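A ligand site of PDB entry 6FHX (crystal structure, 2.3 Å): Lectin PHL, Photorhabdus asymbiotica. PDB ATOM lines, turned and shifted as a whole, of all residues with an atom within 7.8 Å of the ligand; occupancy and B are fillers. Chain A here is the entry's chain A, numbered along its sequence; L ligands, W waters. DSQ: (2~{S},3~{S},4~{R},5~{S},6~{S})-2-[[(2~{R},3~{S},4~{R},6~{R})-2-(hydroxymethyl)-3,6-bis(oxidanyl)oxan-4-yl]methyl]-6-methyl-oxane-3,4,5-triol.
Gly 98 touches the ligand.
Trp 104 touches the ligand (CG to C6, 3.7 Å).
Hydrophobic or aromatic side chains that line the ligand: Trp 104.
Within 4 Å of the ligand: Lys 75, Gly 76, Gln 77, Gly 98, Thr 99 and Trp 104.
The nearest printed residue that does not touch the ligand is Trp 118 (4.03 Å).
An oxygen (O4) of the ligand sits at hydrogen-bond distance from the backbone NH of Thr 99, at 2.8 Å.
The side-chain hydroxyl (OG1) of Thr 99 lies within hydrogen-bond range of an oxygen (O3) of the ligand.
The backbone NH (N) of Gln 77 sits at hydrogen-bond distance from an oxygen (O5) of the ligand.
The backbone carbonyl oxygen (O) of Gln 77 lies within hydrogen-bond range of an oxygen (O4) of the ligand.
O13 of the ligand is in hydrogen-bond range of NZ of Lys 75 (2.9 Å).
O11 of the ligand is in hydrogen-bond range of N of Gly 76.
The backbone NH of Val 54 is in hydrogen-bond range of the backbone carbonyl oxygen of Lys 75, at 2.9 Å.
OG1 of Thr 79 lies within hydrogen-bond range of O of Gly 98 (2.9 Å).
The indole nitrogen of Trp 104 sits at hydrogen-bond distance from the side-chain carboxylate of Asp 100, 3.0 Å away.
O of Ala 96 sits at hydrogen-bond distance from N of Trp 104 (2.8 Å).
Water W1 bridges the backbone NH (N) of Trp 118 (3.4 Å) and the side-chain amide oxygen (OD1) of Asn 117 (3.5 Å).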
ATOM      1  N   LYS A  52     -14.669  -2.252  15.602  1.00  0.00           N
ATOM      2  CA  LYS A  52     -15.836  -3.127  15.377  1.00  0.00           C
ATOM      3  C   LYS A  52     -16.620  -3.513  16.653  1.00  0.00           C
ATOM      4  O   LYS A  52     -17.449  -4.451  16.641  1.00  0.00           O
ATOM      5  CB  LYS A  52     -15.475  -4.380  14.565  1.00  0.00           C
ATOM      6  CG  LYS A  52     -14.690  -4.142  13.278  1.00  0.00           C
ATOM      7  CD  LYS A  52     -15.426  -3.383  12.177  1.00  0.00           C
ATOM      8  CE  LYS A  52     -16.581  -4.143  11.481  1.00  0.00           C
ATOM      9  NZ  LYS A  52     -16.437  -5.615  11.175  1.00  0.00           N
ATOM     10  N   ALA A  53     -16.365  -2.818  17.756  1.00  0.00           N
ATOM     11  CA  ALA A  53     -17.082  -3.054  19.027  1.00  0.00           C
ATOM     12  C   ALA A  53     -18.291  -2.158  19.056  1.00  0.00           C
ATOM     13  O   ALA A  53     -18.358  -1.143  18.350  1.00  0.00           O
ATOM     14  CB  ALA A  53     -16.194  -2.766  20.246  1.00  0.00           C
ATOM     15  N   VAL A  54     -19.261  -2.530  19.880  1.00  0.00           N
ATOM     16  CA  VAL A  54     -20.463  -1.737  20.106  1.00  0.00           C
ATOM     17  C   VAL A  54     -20.184  -0.742  21.211  1.00  0.00           C
ATOM     18  O   VAL A  54     -19.712  -1.133  22.281  1.00  0.00           O
ATOM     19  CB  VAL A  54     -21.649  -2.620  20.513  1.00  0.00           C
ATOM     20  CG1 VAL A  54     -22.897  -1.760  20.722  1.00  0.00           C
ATOM     21  CG2 VAL A  54     -21.898  -3.661  19.439  1.00  0.00           C
ATOM     22  N   LEU A  74     -19.053  -1.531  25.055  1.00  0.00           N
ATOM     23  CA  LEU A  74     -19.588  -2.838  25.432  1.00  0.00           C
ATOM     24  C   LEU A  74     -18.899  -4.004  24.716  1.00  0.00           C
ATOM     25  O   LEU A  74     -19.413  -5.122  24.718  1.00  0.00           O
ATOM     26  CB  LEU A  74     -21.069  -2.889  25.055  1.00  0.00           C
ATOM     27  CG  LEU A  74     -21.923  -1.935  25.871  1.00  0.00           C
ATOM     28  CD1 LEU A  74     -23.293  -1.778  25.201  1.00  0.00           C
ATOM     29  CD2 LEU A  74     -22.029  -2.394  27.323  1.00  0.00           C
ATOM     30  N   LYS A  75     -17.754  -3.716  24.105  1.00  0.00           N
ATOM     31  CA  LYS A  75     -16.928  -4.675  23.389  1.00  0.00           C
ATOM     32  C   LYS A  75     -17.707  -5.405  22.280  1.00  0.00           C
ATOM     33  O   LYS A  75     -18.488  -4.784  21.545  1.00  0.00           O
ATOM     34  CB  LYS A  75     -16.215  -5.567  24.420  1.00  0.00           C
ATOM     35  CG  LYS A  75     -15.515  -4.709  25.469  1.00  0.00           C
ATOM     36  CD  LYS A  75     -14.732  -5.509  26.503  1.00  0.00           C
ATOM     37  CE  LYS A  75     -13.271  -5.708  26.137  1.00  0.00           C
ATOM     38  NZ  LYS A  75     -12.608  -6.653  27.078  1.00  0.00           N
ATOM     39  N   GLY A  76     -17.554  -6.716  22.168  1.00  0.00           N
ATOM     40  CA  GLY A  76     -18.002  -7.437  20.982  1.00  0.00           C
ATOM     41  C   GLY A  76     -17.271  -7.042  19.698  1.00  0.00           C
ATOM     42  O   GLY A  76     -16.513  -6.099  19.669  1.00  0.00           O
ATOM     43  N   GLN A  77     -17.507  -7.846  18.665  1.00  0.00           N
ATOM     44  CA  GLN A  77     -17.027  -7.641  17.298  1.00  0.00           C
ATOM     45  C   GLN A  77     -18.244  -7.888  16.440  1.00  0.00           C
ATOM     46  O   GLN A  77     -18.711  -9.017  16.415  1.00  0.00           O
ATOM     47  CB  GLN A  77     -15.948  -8.670  16.911  1.00  0.00           C
ATOM     48  CG  GLN A  77     -14.624  -8.521  17.644  1.00  0.00           C
ATOM     49  CD  GLN A  77     -13.781  -7.389  17.070  1.00  0.00           C
ATOM     50  OE1 GLN A  77     -12.996  -7.615  16.127  1.00  0.00           O
ATOM     51  NE2 GLN A  77     -13.946  -6.174  17.612  1.00  0.00           N
ATOM     52  N   VAL A  78     -18.757  -6.854  15.760  1.00  0.00           N
ATOM     53  CA  VAL A  78     -20.039  -6.976  15.035  1.00  0.00           C
ATOM     54  C   VAL A  78     -19.907  -6.803  13.533  1.00  0.00           C
ATOM     55  O   VAL A  78     -19.089  -6.048  13.071  1.00  0.00           O
ATOM     56  CB  VAL A  78     -21.154  -6.055  15.608  1.00  0.00           C
ATOM     57  CG1 VAL A  78     -21.413  -6.381  17.076  1.00  0.00           C
ATOM     58  CG2 VAL A  78     -20.839  -4.591  15.410  1.00  0.00           C
ATOM     59  N   THR A  79     -20.737  -7.527  12.780  1.00  0.00           N
ATOM     60  CA  THR A  79     -20.798  -7.493  11.314  1.00  0.00           C
ATOM     61  C   THR A  79     -22.181  -7.042  10.801  1.00  0.00           C
ATOM     62  O   THR A  79     -22.585  -7.378   9.675  1.00  0.00           O
ATOM     63  CB  THR A  79     -20.536  -8.907  10.768  1.00  0.00           C
ATOM     64  OG1 THR A  79     -21.575  -9.777  11.238  1.00  0.00           O
ATOM     65  CG2 THR A  79     -19.146  -9.435  11.263  1.00  0.00           C
ATOM     66  N   ALA A  96     -26.977  -7.908  17.561  1.00  0.00           N
ATOM     67  CA  ALA A  96     -26.098  -7.673  16.412  1.00  0.00           C
ATOM     68  C   ALA A  96     -25.610  -8.982  15.878  1.00  0.00           C
ATOM     69  O   ALA A  96     -25.403  -9.952  16.623  1.00  0.00           O
ATOM     70  CB  ALA A  96     -24.926  -6.782  16.792  1.00  0.00           C
ATOM     71  N   ARG A  97     -25.417  -9.019  14.571  1.00  0.00           N
ATOM     72  CA  ARG A  97     -24.742 -10.124  13.938  1.00  0.00           C
ATOM     73  C   ARG A  97     -23.276 -10.182  14.328  1.00  0.00           C
ATOM     74  O   ARG A  97     -22.586  -9.170  14.323  1.00  0.00           O
ATOM     75  CB  ARG A  97     -24.862 -10.016  12.451  1.00  0.00           C
ATOM     76  CG  ARG A  97     -24.466 -11.330  11.784  1.00  0.00           C
ATOM     77  CD  ARG A  97     -24.616 -11.258  10.292  1.00  0.00           C
ATOM     78  NE  ARG A  97     -23.757 -10.249   9.684  1.00  0.00           N
ATOM     79  CZ  ARG A  97     -23.348 -10.299   8.419  1.00  0.00           C
ATOM     80  NH1 ARG A  97     -23.724 -11.313   7.648  1.00  0.00           N
ATOM     81  NH2 ARG A  97     -22.584  -9.348   7.928  1.00  0.00           N
ATOM     82  N   GLY A  98     -22.794 -11.382  14.628  1.00  0.00           N
ATOM     83  CA  GLY A  98     -21.386 -11.618  14.965  1.00  0.00           C
ATOM     84  C   GLY A  98     -20.457 -11.984  13.831  1.00  0.00           C
ATOM     85  O   GLY A  98     -20.858 -12.196  12.684  1.00  0.00           O
ATOM     86  N   THR A  99     -19.188 -12.124  14.198  1.00  0.00           N
ATOM     87  CA  THR A  99     -18.107 -12.550  13.315  1.00  0.00           C
ATOM     88  C   THR A  99     -18.313 -13.962  12.696  1.00  0.00           C
ATOM     89  O   THR A  99     -17.744 -14.281  11.652  1.00  0.00           O
ATOM     90  CB  THR A  99     -16.753 -12.490  14.074  1.00  0.00           C
ATOM     91  OG1 THR A  99     -16.806 -13.288  15.267  1.00  0.00           O
ATOM     92  CG2 THR A  99     -16.392 -11.039  14.435  1.00  0.00           C
ATOM     93  N   ASP A 100     -19.096 -14.802  13.388  1.00  0.00           N
ATOM     94  CA  ASP A 100     -19.527 -16.119  12.921  1.00  0.00           C
ATOM     95  C   ASP A 100     -20.933 -16.161  12.249  1.00  0.00           C
ATOM     96  O   ASP A 100     -21.495 -17.246  12.039  1.00  0.00           O
ATOM     97  CB  ASP A 100     -19.485 -17.079  14.107  1.00  0.00           C
ATOM     98  CG  ASP A 100     -20.350 -16.609  15.312  1.00  0.00           C
ATOM     99  OD1 ASP A 100     -21.100 -15.638  15.199  1.00  0.00           O
ATOM    100  OD2 ASP A 100     -20.267 -17.229  16.400  1.00  0.00           O
ATOM    101  N   ASN A 101     -21.500 -14.971  11.974  1.00  0.00           N
ATOM    102  CA  ASN A 101     -22.834 -14.794  11.372  1.00  0.00           C
ATOM    103  C   ASN A 101     -24.049 -15.238  12.199  1.00  0.00           C
ATOM    104  O   ASN A 101     -25.173 -15.299  11.678  1.00  0.00           O
ATOM    105  CB  ASN A 101     -22.855 -15.381   9.964  1.00  0.00           C
ATOM    106  CG  ASN A 101     -21.954 -14.622   9.015  1.00  0.00           C
ATOM    107  OD1 ASN A 101     -21.868 -13.392   9.091  1.00  0.00           O
ATOM    108  ND2 ASN A 101     -21.244 -15.347   8.137  1.00  0.00           N
ATOM    109  N   ALA A 102     -23.817 -15.513  13.486  1.00  0.00           N
ATOM    110  CA  ALA A 102     -24.880 -15.805  14.407  1.00  0.00           C
ATOM    111  C   ALA A 102     -25.383 -14.500  14.922  1.00  0.00           C
ATOM    112  O   ALA A 102     -24.684 -13.475  14.865  1.00  0.00           O
ATOM    113  CB  ALA A 102     -24.387 -16.662  15.560  1.00  0.00           C
ATOM    114  N   LEU A 103     -26.619 -14.569  15.429  1.00  0.00           N
ATOM    115  CA  LEU A 103     -27.213 -13.474  16.143  1.00  0.00           C
ATOM    116  C   LEU A 103     -26.600 -13.524  17.508  1.00  0.00           C
ATOM    117  O   LEU A 103     -26.717 -14.569  18.172  1.00  0.00           O
ATOM    118  CB  LEU A 103     -28.726 -13.669  16.238  1.00  0.00           C
ATOM    119  CG  LEU A 103     -29.593 -12.632  16.965  1.00  0.00           C
ATOM    120  CD1 LEU A 103     -29.574 -11.300  16.221  1.00  0.00           C
ATOM    121  CD2 LEU A 103     -31.009 -13.172  17.082  1.00  0.00           C
ATOM    122  N   TRP A 104     -25.970 -12.423  17.923  1.00  0.00           N
ATOM    123  CA  TRP A 104     -25.500 -12.263  19.319  1.00  0.00           C
ATOM    124  C   TRP A 104     -26.279 -11.154  20.034  1.00  0.00           C
ATOM    125  O   TRP A 104     -26.882 -10.275  19.393  1.00  0.00           O
ATOM    126  CB  TRP A 104     -23.992 -11.912  19.398  1.00  0.00           C
ATOM    127  CG  TRP A 104     -23.114 -13.049  19.022  1.00  0.00           C
ATOM    128  CD1 TRP A 104     -23.034 -13.614  17.784  1.00  0.00           C
ATOM    129  CD2 TRP A 104     -22.186 -13.759  19.850  1.00  0.00           C
ATOM    130  NE1 TRP A 104     -22.112 -14.614  17.794  1.00  0.00           N
ATOM    131  CE2 TRP A 104     -21.594 -14.757  19.045  1.00  0.00           C
ATOM    132  CE3 TRP A 104     -21.772 -13.640  21.173  1.00  0.00           C
ATOM    133  CZ2 TRP A 104     -20.607 -15.667  19.528  1.00  0.00           C
ATOM    134  CZ3 TRP A 104     -20.799 -14.560  21.679  1.00  0.00           C
ATOM    135  CH2 TRP A 104     -20.236 -15.539  20.840  1.00  0.00           C
ATOM    136  N   HIS A 105     -26.250 -11.199  21.361  1.00  0.00           N
ATOM    137  CA  HIS A 105     -26.903 -10.215  22.163  1.00  0.00           C
ATOM    138  C   HIS A 105     -26.210  -9.979  23.464  1.00  0.00           C
ATOM    139  O   HIS A 105     -25.355 -10.766  23.876  1.00  0.00           O
ATOM    140  CB  HIS A 105     -28.398 -10.487  22.368  1.00  0.00           C
ATOM    141  CG  HIS A 105     -28.725 -11.690  23.215  1.00  0.00           C
ATOM    142  ND1 HIS A 105     -29.773 -11.700  24.102  1.00  0.00           N
ATOM    143  CD2 HIS A 105     -28.166 -12.923  23.267  1.00  0.00           C
ATOM    144  CE1 HIS A 105     -29.846 -12.883  24.673  1.00  0.00           C
ATOM    145  NE2 HIS A 105     -28.877 -13.644  24.198  1.00  0.00           N
ATOM    146  N   ILE A 106     -26.541  -8.825  24.037  1.00  0.00           N
ATOM    147  CA  ILE A 106     -26.028  -8.355  25.293  1.00  0.00           C
ATOM    148  C   ILE A 106     -27.119  -7.491  25.920  1.00  0.00           C
ATOM    149  O   ILE A 106     -27.819  -6.750  25.240  1.00  0.00           O
ATOM    150  CB  ILE A 106     -24.678  -7.613  25.093  1.00  0.00           C
ATOM    151  CG1 ILE A 106     -23.984  -7.390  26.444  1.00  0.00           C
ATOM    152  CG2 ILE A 106     -24.853  -6.296  24.311  1.00  0.00           C
ATOM    153  CD1 ILE A 106     -22.601  -6.758  26.325  1.00  0.00           C
ATOM    154  N   ASN A 117     -22.367 -10.134  29.622  1.00  0.00           N
ATOM    155  CA  ASN A 117     -21.520 -10.451  28.492  1.00  0.00           C
ATOM    156  C   ASN A 117     -22.340 -10.779  27.252  1.00  0.00           C
ATOM    157  O   ASN A 117     -23.493 -11.163  27.371  1.00  0.00           O
ATOM    158  CB  ASN A 117     -20.651 -11.662  28.825  1.00  0.00           C
ATOM    159  CG  ASN A 117     -19.567 -11.333  29.828  1.00  0.00           C
ATOM    160  OD1 ASN A 117     -18.986 -10.241  29.807  1.00  0.00           O
ATOM    161  ND2 ASN A 117     -19.283 -12.272  30.726  1.00  0.00           N
ATOM    162  N   TRP A 118     -21.742 -10.591  26.083  1.00  0.00           N
ATOM    163  CA  TRP A 118     -22.325 -11.019  24.834  1.00  0.00           C
ATOM    164  C   TRP A 118     -22.562 -12.529  24.832  1.00  0.00           C
ATOM    165  O   TRP A 118     -21.664 -13.268  25.210  1.00  0.00           O
ATOM    166  CB  TRP A 118     -21.354 -10.721  23.694  1.00  0.00           C
ATOM    167  CG  TRP A 118     -21.281  -9.307  23.327  1.00  0.00           C
ATOM    168  CD1 TRP A 118     -20.392  -8.423  23.772  1.00  0.00           C
ATOM    169  CD2 TRP A 118     -22.144  -8.615  22.423  1.00  0.00           C
ATOM    170  NE1 TRP A 118     -20.634  -7.185  23.223  1.00  0.00           N
ATOM    171  CE2 TRP A 118     -21.718  -7.292  22.380  1.00  0.00           C
ATOM    172  CE3 TRP A 118     -23.229  -9.000  21.633  1.00  0.00           C
ATOM    173  CZ2 TRP A 118     -22.352  -6.320  21.567  1.00  0.00           C
ATOM    174  CZ3 TRP A 118     -23.875  -8.040  20.858  1.00  0.00           C
ATOM    175  CH2 TRP A 118     -23.428  -6.724  20.816  1.00  0.00           C
ATOM    176  N   GLN A 119     -23.747 -12.965  24.403  1.00  0.00           N
ATOM    177  CA  GLN A 119     -24.018 -14.381  24.216  1.00  0.00           C
ATOM    178  C   GLN A 119     -24.607 -14.620  22.831  1.00  0.00           C
ATOM    179  O   GLN A 119     -25.200 -13.746  22.230  1.00  0.00           O
ATOM    180  CB  GLN A 119     -24.955 -14.914  25.304  1.00  0.00           C
ATOM    181  CG  GLN A 119     -24.311 -15.019  26.706  1.00  0.00           C
ATOM    182  CD  GLN A 119     -25.106 -15.890  27.697  1.00  0.00           C
ATOM    183  OE1 GLN A 119     -26.067 -16.597  27.320  1.00  0.00           O
ATOM    184  NE2 GLN A 119     -24.714 -15.828  28.966  1.00  0.00           N
ATOM    185  N   SER A 120     -24.416 -15.824  22.314  1.00  0.00           N
ATOM    186  CA  SER A 120     -24.845 -16.164  20.989  1.00  0.00           C
ATOM    187  C   SER A 120     -26.219 -16.783  21.056  1.00  0.00           C
ATOM    188  O   SER A 120     -26.471 -17.654  21.869  1.00  0.00           O
ATOM    189  CB  SER A 120     -23.873 -17.130  20.326  1.00  0.00           C
ATOM    190  OG  SER A 120     -24.380 -17.595  19.091  1.00  0.00           O
HETATM  191  C8  DSQ L   1     -15.515 -12.994  24.709  1.00  0.00           C
HETATM  192  C9  DSQ L   1     -16.676 -12.964  23.682  1.00  0.00           C
HETATM  193  C10 DSQ L   1     -16.583 -11.723  22.762  1.00  0.00           C
HETATM  194  C11 DSQ L   1     -16.476 -10.479  23.639  1.00  0.00           C
HETATM  195  C12 DSQ L   1     -15.409 -10.625  24.740  1.00  0.00           C
HETATM  196  C13 DSQ L   1     -15.491  -9.451  25.725  1.00  0.00           C
HETATM  197  O8  DSQ L   1     -15.524 -14.119  25.609  1.00  0.00           O
HETATM  198  O12 DSQ L   1     -15.612 -11.817  25.501  1.00  0.00           O
HETATM  199  O13 DSQ L   1     -14.229  -8.829  25.977  1.00  0.00           O
HETATM  200  O11 DSQ L   1     -16.160  -9.375  22.782  1.00  0.00           O
HETATM  201  C7  DSQ L   1     -17.729 -11.599  21.721  1.00  0.00           C
HETATM  202  C1  DSQ L   1     -17.353 -11.079  20.294  1.00  0.00           C
HETATM  203  C2  DSQ L   1     -16.869 -12.143  19.280  1.00  0.00           C
HETATM  204  O2  DSQ L   1     -15.901 -13.022  19.858  1.00  0.00           O
HETATM  205  C3  DSQ L   1     -17.983 -13.003  18.708  1.00  0.00           C
HETATM  206  O3  DSQ L   1     -17.477 -13.881  17.682  1.00  0.00           O
HETATM  207  C4  DSQ L   1     -19.113 -12.153  18.134  1.00  0.00           C
HETATM  208  O4  DSQ L   1     -18.683 -11.581  16.862  1.00  0.00           O
HETATM  209  C5  DSQ L   1     -19.555 -11.157  19.233  1.00  0.00           C
HETATM  210  O5  DSQ L   1     -18.451 -10.356  19.712  1.00  0.00           O
HETATM  211  C6  DSQ L   1     -20.718 -10.260  18.746  1.00  0.00           C
HETATM  212  O   HOH W   1     -18.563  -9.468  26.469  1.00  0.00           O
